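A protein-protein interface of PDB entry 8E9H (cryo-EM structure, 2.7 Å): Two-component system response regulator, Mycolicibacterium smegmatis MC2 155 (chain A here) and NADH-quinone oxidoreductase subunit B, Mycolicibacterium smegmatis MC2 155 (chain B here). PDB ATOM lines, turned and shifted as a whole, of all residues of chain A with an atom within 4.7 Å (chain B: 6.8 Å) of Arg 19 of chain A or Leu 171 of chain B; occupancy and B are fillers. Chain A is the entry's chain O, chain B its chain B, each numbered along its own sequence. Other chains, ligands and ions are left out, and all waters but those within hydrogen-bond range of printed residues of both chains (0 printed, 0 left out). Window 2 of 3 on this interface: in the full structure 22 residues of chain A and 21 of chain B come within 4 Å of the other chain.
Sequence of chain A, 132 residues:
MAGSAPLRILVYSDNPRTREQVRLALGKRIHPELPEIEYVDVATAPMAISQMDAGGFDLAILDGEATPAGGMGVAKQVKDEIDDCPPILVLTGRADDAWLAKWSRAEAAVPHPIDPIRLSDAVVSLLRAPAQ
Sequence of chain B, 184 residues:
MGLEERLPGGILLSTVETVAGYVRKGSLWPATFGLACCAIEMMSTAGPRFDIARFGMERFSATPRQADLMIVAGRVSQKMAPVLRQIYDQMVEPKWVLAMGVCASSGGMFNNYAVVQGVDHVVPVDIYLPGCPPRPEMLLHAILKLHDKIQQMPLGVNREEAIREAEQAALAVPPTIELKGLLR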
ATOM      1  N   VAL A  11     -35.069  19.527   4.356  1.00  0.00           N
ATOM      2  CA  VAL A  11     -34.500  19.001   3.124  1.00  0.00           C
ATOM      3  C   VAL A  11     -33.012  19.313   3.169  1.00  0.00           C
ATOM      4  O   VAL A  11     -32.611  20.480   3.114  1.00  0.00           O
ATOM      5  CB  VAL A  11     -35.157  19.598   1.879  1.00  0.00           C
ATOM      6  CG1 VAL A  11     -34.586  18.961   0.632  1.00  0.00           C
ATOM      7  CG2 VAL A  11     -36.656  19.407   1.937  1.00  0.00           C
ATOM      8  N   SER A  13     -29.363  18.735   1.406  1.00  0.00           N
ATOM      9  CA  SER A  13     -28.614  18.305   0.238  1.00  0.00           C
ATOM     10  C   SER A  13     -27.670  19.419  -0.174  1.00  0.00           C
ATOM     11  O   SER A  13     -28.079  20.577  -0.279  1.00  0.00           O
ATOM     12  CB  SER A  13     -29.545  17.947  -0.921  1.00  0.00           C
ATOM     13  OG  SER A  13     -28.813  17.387  -1.994  1.00  0.00           O
ATOM     14  N   ASP A  14     -26.407  19.061  -0.401  1.00  0.00           N
ATOM     15  CA  ASP A  14     -25.459  20.034  -0.928  1.00  0.00           C
ATOM     16  C   ASP A  14     -25.877  20.501  -2.313  1.00  0.00           C
ATOM     17  O   ASP A  14     -25.556  21.621  -2.723  1.00  0.00           O
ATOM     18  CB  ASP A  14     -24.059  19.427  -0.969  1.00  0.00           C
ATOM     19  N   ASN A  15     -26.601  19.657  -3.046  1.00  0.00           N
ATOM     20  CA  ASN A  15     -27.006  19.969  -4.408  1.00  0.00           C
ATOM     21  C   ASN A  15     -28.314  20.745  -4.371  1.00  0.00           C
ATOM     22  O   ASN A  15     -29.333  20.192  -3.932  1.00  0.00           O
ATOM     23  CB  ASN A  15     -27.170  18.693  -5.214  1.00  0.00           C
ATOM     24  CG  ASN A  15     -27.493  18.955  -6.665  1.00  0.00           C
ATOM     25  OD1 ASN A  15     -28.119  19.956  -7.004  1.00  0.00           O
ATOM     26  ND2 ASN A  15     -27.067  18.050  -7.534  1.00  0.00           N
ATOM     27  N   PRO A  16     -28.350  22.002  -4.819  1.00  0.00           N
ATOM     28  CA  PRO A  16     -29.631  22.722  -4.828  1.00  0.00           C
ATOM     29  C   PRO A  16     -30.668  22.091  -5.731  1.00  0.00           C
ATOM     30  O   PRO A  16     -31.868  22.263  -5.493  1.00  0.00           O
ATOM     31  CB  PRO A  16     -29.238  24.124  -5.307  1.00  0.00           C
ATOM     32  CG  PRO A  16     -27.999  23.923  -6.074  1.00  0.00           C
ATOM     33  CD  PRO A  16     -27.265  22.819  -5.384  1.00  0.00           C
ATOM     34  N   ARG A  17     -30.251  21.366  -6.768  1.00  0.00           N
ATOM     35  CA  ARG A  17     -31.225  20.748  -7.658  1.00  0.00           C
ATOM     36  C   ARG A  17     -31.935  19.580  -6.996  1.00  0.00           C
ATOM     37  O   ARG A  17     -33.119  19.355  -7.257  1.00  0.00           O
ATOM     38  CB  ARG A  17     -30.553  20.301  -8.952  1.00  0.00           C
ATOM     39  CG  ARG A  17     -29.756  21.394  -9.641  1.00  0.00           C
ATOM     40  CD  ARG A  17     -30.593  22.640  -9.898  1.00  0.00           C
ATOM     41  NE  ARG A  17     -29.771  23.747 -10.372  1.00  0.00           N
ATOM     42  CZ  ARG A  17     -29.629  24.911  -9.750  1.00  0.00           C
ATOM     43  NH1 ARG A  17     -30.257  25.178  -8.617  1.00  0.00           N
ATOM     44  NH2 ARG A  17     -28.831  25.833 -10.280  1.00  0.00           N
ATOM     45  N   THR A  18     -31.247  18.823  -6.143  1.00  0.00           N
ATOM     46  CA  THR A  18     -31.941  17.783  -5.394  1.00  0.00           C
ATOM     47  C   THR A  18     -32.971  18.389  -4.453  1.00  0.00           C
ATOM     48  O   THR A  18     -34.081  17.865  -4.318  1.00  0.00           O
ATOM     49  CB  THR A  18     -30.947  16.926  -4.618  1.00  0.00           C
ATOM     50  OG1 THR A  18     -30.270  17.737  -3.651  1.00  0.00           O
ATOM     51  CG2 THR A  18     -29.935  16.299  -5.557  1.00  0.00           C
ATOM     52  N   ARG A  19     -32.627  19.498  -3.798  1.00  0.00           N
ATOM     53  CA  ARG A  19     -33.604  20.179  -2.960  1.00  0.00           C
ATOM     54  C   ARG A  19     -34.782  20.672  -3.787  1.00  0.00           C
ATOM     55  O   ARG A  19     -35.935  20.563  -3.360  1.00  0.00           O
ATOM     56  CB  ARG A  19     -32.949  21.343  -2.222  1.00  0.00           C
ATOM     57  CG  ARG A  19     -31.765  20.938  -1.374  1.00  0.00           C
ATOM     58  CD  ARG A  19     -31.442  22.002  -0.354  1.00  0.00           C
ATOM     59  NE  ARG A  19     -31.237  23.301  -0.980  1.00  0.00           N
ATOM     60  CZ  ARG A  19     -30.058  23.777  -1.356  1.00  0.00           C
ATOM     61  NH1 ARG A  19     -28.945  23.080  -1.196  1.00  0.00           N
ATOM     62  NH2 ARG A  19     -29.995  24.981  -1.914  1.00  0.00           N
ATOM     63  N   GLU A  20     -34.512  21.218  -4.972  1.00  0.00           N
ATOM     64  CA  GLU A  20     -35.595  21.679  -5.831  1.00  0.00           C
ATOM     65  C   GLU A  20     -36.498  20.523  -6.234  1.00  0.00           C
ATOM     66  O   GLU A  20     -37.725  20.645  -6.220  1.00  0.00           O
ATOM     67  CB  GLU A  20     -35.021  22.373  -7.065  1.00  0.00           C
ATOM     68  N   GLN A  21     -35.909  19.382  -6.586  1.00  0.00           N
ATOM     69  CA  GLN A  21     -36.715  18.228  -6.967  1.00  0.00           C
ATOM     70  C   GLN A  21     -37.549  17.729  -5.797  1.00  0.00           C
ATOM     71  O   GLN A  21     -38.713  17.357  -5.972  1.00  0.00           O
ATOM     72  CB  GLN A  21     -35.822  17.108  -7.491  1.00  0.00           C
ATOM     73  CG  GLN A  21     -35.359  17.307  -8.915  1.00  0.00           C
ATOM     74  CD  GLN A  21     -34.342  16.272  -9.334  1.00  0.00           C
ATOM     75  OE1 GLN A  21     -34.259  15.195  -8.745  1.00  0.00           O
ATOM     76  NE2 GLN A  21     -33.557  16.594 -10.353  1.00  0.00           N
ATOM     77  N   VAL A  22     -36.968  17.693  -4.599  1.00  0.00           N
ATOM     78  CA  VAL A  22     -37.726  17.253  -3.432  1.00  0.00           C
ATOM     79  C   VAL A  22     -38.883  18.204  -3.169  1.00  0.00           C
ATOM     80  O   VAL A  22     -40.018  17.782  -2.930  1.00  0.00           O
ATOM     81  CB  VAL A  22     -36.805  17.137  -2.206  1.00  0.00           C
ATOM     82  CG1 VAL A  22     -37.628  17.063  -0.937  1.00  0.00           C
ATOM     83  CG2 VAL A  22     -35.917  15.920  -2.331  1.00  0.00           C
ATOM     84  N   ARG A  23     -38.615  19.496  -3.216  1.00  0.00           N
ATOM     85  CA  ARG A  23     -39.628  20.511  -2.978  1.00  0.00           C
ATOM     86  C   ARG A  23     -40.608  20.628  -4.104  1.00  0.00           C
ATOM     87  O   ARG A  23     -41.612  21.327  -3.959  1.00  0.00           O
ATOM     88  CB  ARG A  23     -38.940  21.852  -2.731  1.00  0.00           C
ATOM     89  CG  ARG A  23     -39.765  22.838  -1.934  1.00  0.00           C
ATOM     90  CD  ARG A  23     -38.883  23.893  -1.299  1.00  0.00           C
ATOM     91  NE  ARG A  23     -38.124  24.635  -2.299  1.00  0.00           N
ATOM     92  CZ  ARG A  23     -36.836  24.457  -2.559  1.00  0.00           C
ATOM     93  NH1 ARG A  23     -36.116  23.552  -1.917  1.00  0.00           N
ATOM     94  NH2 ARG A  23     -36.256  25.204  -3.494  1.00  0.00           N
ATOM     95  N   ASP A  41     -34.699  24.354   3.822  1.00  0.00           N
ATOM     96  CA  ASP A  41     -33.542  23.876   3.082  1.00  0.00           C
ATOM     97  C   ASP A  41     -32.272  24.077   3.892  1.00  0.00           C
ATOM     98  O   ASP A  41     -32.039  25.146   4.460  1.00  0.00           O
ATOM     99  CB  ASP A  41     -33.426  24.607   1.748  1.00  0.00           C
ATOM    100  CG  ASP A  41     -34.286  23.988   0.670  1.00  0.00           C
ATOM    101  OD1 ASP A  41     -35.306  23.358   1.012  1.00  0.00           O
ATOM    102  OD2 ASP A  41     -33.939  24.130  -0.521  1.00  0.00           O
ATOM    103  N   VAL A  42     -31.446  23.037   3.946  1.00  0.00           N
ATOM    104  CA  VAL A  42     -30.145  23.102   4.598  1.00  0.00           C
ATOM    105  C   VAL A  42     -29.121  22.463   3.677  1.00  0.00           C
ATOM    106  O   VAL A  42     -29.354  21.383   3.127  1.00  0.00           O
ATOM    107  CB  VAL A  42     -30.157  22.408   5.972  1.00  0.00           C
ATOM    108  CG1 VAL A  42     -31.055  23.160   6.926  1.00  0.00           C
ATOM    109  CG2 VAL A  42     -30.606  20.969   5.835  1.00  0.00           C
ATOM    110  N   ALA A  43     -27.985  23.133   3.506  1.00  0.00           N
ATOM    111  CA  ALA A  43     -26.938  22.661   2.613  1.00  0.00           C
ATOM    112  C   ALA A  43     -25.740  22.078   3.343  1.00  0.00           C
ATOM    113  O   ALA A  43     -24.933  21.382   2.721  1.00  0.00           O
ATOM    114  CB  ALA A  43     -26.462  23.803   1.713  1.00  0.00           C
ATOM    115  N   ARG B 164     -24.105  29.686  10.434  1.00  0.00           N
ATOM    116  CA  ARG B 164     -25.145  30.347   9.652  1.00  0.00           C
ATOM    117  C   ARG B 164     -24.583  30.922   8.356  1.00  0.00           C
ATOM    118  O   ARG B 164     -25.201  30.795   7.293  1.00  0.00           O
ATOM    119  CB  ARG B 164     -25.806  31.444  10.482  1.00  0.00           C
ATOM    120  N   ALA B 166     -21.823  29.980   6.705  1.00  0.00           N
ATOM    121  CA  ALA B 166     -21.458  28.885   5.818  1.00  0.00           C
ATOM    122  C   ALA B 166     -22.694  28.278   5.175  1.00  0.00           C
ATOM    123  O   ALA B 166     -22.662  27.881   4.006  1.00  0.00           O
ATOM    124  CB  ALA B 166     -20.681  27.821   6.588  1.00  0.00           C
ATOM    125  N   GLU B 167     -23.790  28.190   5.924  1.00  0.00           N
ATOM    126  CA  GLU B 167     -25.045  27.743   5.337  1.00  0.00           C
ATOM    127  C   GLU B 167     -25.481  28.680   4.222  1.00  0.00           C
ATOM    128  O   GLU B 167     -25.785  28.242   3.108  1.00  0.00           O
ATOM    129  CB  GLU B 167     -26.123  27.663   6.414  1.00  0.00           C
ATOM    130  CG  GLU B 167     -27.484  27.302   5.873  1.00  0.00           C
ATOM    131  CD  GLU B 167     -27.499  25.923   5.269  1.00  0.00           C
ATOM    132  OE1 GLU B 167     -26.663  25.090   5.676  1.00  0.00           O
ATOM    133  OE2 GLU B 167     -28.331  25.675   4.376  1.00  0.00           O
ATOM    134  N   GLN B 168     -25.513  29.981   4.507  1.00  0.00           N
ATOM    135  CA  GLN B 168     -25.950  30.939   3.498  1.00  0.00           C
ATOM    136  C   GLN B 168     -25.102  30.827   2.240  1.00  0.00           C
ATOM    137  O   GLN B 168     -25.621  30.917   1.121  1.00  0.00           O
ATOM    138  CB  GLN B 168     -25.889  32.357   4.062  1.00  0.00           C
ATOM    139  N   ALA B 169     -23.795  30.628   2.401  1.00  0.00           N
ATOM    140  CA  ALA B 169     -22.921  30.505   1.239  1.00  0.00           C
ATOM    141  C   ALA B 169     -23.176  29.203   0.489  1.00  0.00           C
ATOM    142  O   ALA B 169     -23.255  29.190  -0.744  1.00  0.00           O
ATOM    143  CB  ALA B 169     -21.460  30.596   1.672  1.00  0.00           C
ATOM    144  N   ALA B 170     -23.309  28.095   1.218  1.00  0.00           N
ATOM    145  CA  ALA B 170     -23.426  26.793   0.572  1.00  0.00           C
ATOM    146  C   ALA B 170     -24.760  26.630  -0.139  1.00  0.00           C
ATOM    147  O   ALA B 170     -24.854  25.876  -1.114  1.00  0.00           O
ATOM    148  CB  ALA B 170     -23.241  25.682   1.602  1.00  0.00           C
ATOM    149  N   LEU B 171     -25.803  27.316   0.328  1.00  0.00           N
ATOM    150  CA  LEU B 171     -27.112  27.163  -0.295  1.00  0.00           C
ATOM    151  C   LEU B 171     -27.108  27.639  -1.740  1.00  0.00           C
ATOM    152  O   LEU B 171     -27.984  27.251  -2.520  1.00  0.00           O
ATOM    153  CB  LEU B 171     -28.164  27.929   0.503  1.00  0.00           C
ATOM    154  CG  LEU B 171     -28.707  27.214   1.739  1.00  0.00           C
ATOM    155  CD1 LEU B 171     -29.393  28.201   2.664  1.00  0.00           C
ATOM    156  CD2 LEU B 171     -29.662  26.109   1.343  1.00  0.00           C
ATOM    157  N   ALA B 172     -26.141  28.471  -2.117  1.00  0.00           N
ATOM    158  CA  ALA B 172     -26.160  29.106  -3.428  1.00  0.00           C
ATOM    159  C   ALA B 172     -25.266  28.418  -4.447  1.00  0.00           C
ATOM    160  O   ALA B 172     -25.521  28.529  -5.651  1.00  0.00           O
ATOM    161  CB  ALA B 172     -25.740  30.572  -3.302  1.00  0.00           C
ATOM    162  N   VAL B 173     -24.232  27.713  -4.007  1.00  0.00           N
ATOM    163  CA  VAL B 173     -23.260  27.161  -4.959  1.00  0.00           C
ATOM    164  C   VAL B 173     -23.969  26.185  -5.891  1.00  0.00           C
ATOM    165  O   VAL B 173     -24.664  25.273  -5.411  1.00  0.00           O
ATOM    166  CB  VAL B 173     -22.114  26.476  -4.213  1.00  0.00           C
ATOM    167  CG1 VAL B 173     -21.461  27.446  -3.243  1.00  0.00           C
ATOM    168  CG2 VAL B 173     -22.605  25.236  -3.489  1.00  0.00           C
ATOM    169  N   PRO B 174     -23.842  26.330  -7.213  1.00  0.00           N
ATOM    170  CA  PRO B 174     -24.451  25.350  -8.106  1.00  0.00           C
ATOM    171  C   PRO B 174     -23.726  24.020  -8.019  1.00  0.00           C
ATOM    172  O   PRO B 174     -22.540  23.967  -7.652  1.00  0.00           O
ATOM    173  CB  PRO B 174     -24.288  25.988  -9.498  1.00  0.00           C
ATOM    174  CG  PRO B 174     -24.010  27.422  -9.240  1.00  0.00           C
ATOM    175  CD  PRO B 174     -23.255  27.451  -7.962  1.00  0.00           C
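The backbone NH (N) of Ala 43 of chain A is in hydrogen-bond range of the side-chain carboxylate (OE2) of Glu 167 of chain B (2.7 Å). The backbone carbonyl oxygen of Leu 171 of chain B lies within hydrogen-bond range of the guanidinium group of Arg 19 of chain A, 3.1 Å away.
The backbone carbonyl oxygen (O) of Val 42 of chain A is in hydrogen-bond range of the backbone NH (N) of Ser 13 of chain A. The backbone carbonyl oxygen of Val 11 of chain A is in hydrogen-bond range of the backbone NH of Val 42 of chain A (2.9 Å). The backbone carbonyl oxygen (O) of Arg 19 of chain A sits at hydrogen-bond distance from the guanidinium group (NH1) of Arg 23 of chain A. OD2 of Asp 41 of chain A lies within salt-bridge range of NH1 of Arg 23 of chain A, 2.6 Å away. The guanidinium group (NE) of Arg 19 of chain A is in salt-bridge range of the side-chain carboxylate (OD2) of Asp 41 of chain A (2.9 Å). The backbone carbonyl oxygen (O) of Ser 13 of chain A sits at hydrogen-bond distance from the guanidinium group (NH1) of Arg 19 of chain A (2.8 Å).
Among the printed residues, merely in contact across the chains: Pro 16 of chain A with Val 173 of chain B, Asp 41 of chain A with Glu 167 of chain B, Val 42 of chain A with Glu 167 of chain B, Ala 43 of chain A with Ala 170 of chain B and Ala 43 of chain A with Leu 171 of chain B.
Ser 13 of chain A touches none of the printed residues of chain B. Printed residues of chain B within 4 Å of Pro 16 of chain A: Val 173. Arg 19 of chain A touches one residue of chain B. Of the printed residues of chain B, Asp 41 of chain A touches Glu 167 (3.7 Å). Of the printed residues of chain A, Glu 167 of chain B touches Asp 41, Val 42 and Ala 43. Printed residues of chain A within 4 Å of Ala 170 of chain B: Ala 43. Leu 171 of chain B touches two residues of chain A. Printed residues of chain A within 4 Å of Val 173 of chain B: Pro 16 (3.6 Å). The nearest residue of chain A that does not touch Leu 171 of chain B is Asp 41 of chain A (4.04 Å). The nearest printed residue of chain A that does not touch Glu 167 of chain B is Arg 19 of chain A (6.2 Å).
Of the 10 printed residues of chain B, 4 touch a printed residue of chain A. Hydrophobic or aromatic side chains of chain B within 4 Å of the printed part of chain A: Ala 170 and Leu 171. Of the 15 printed residues of chain A, 5 touch a printed residue of chain B. Hydrophobic or aromatic side chains of chain A that line the printed part of chain B: Pro 16 and Ala 43. Among the printed residues, 7 pairs touch across the chains.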
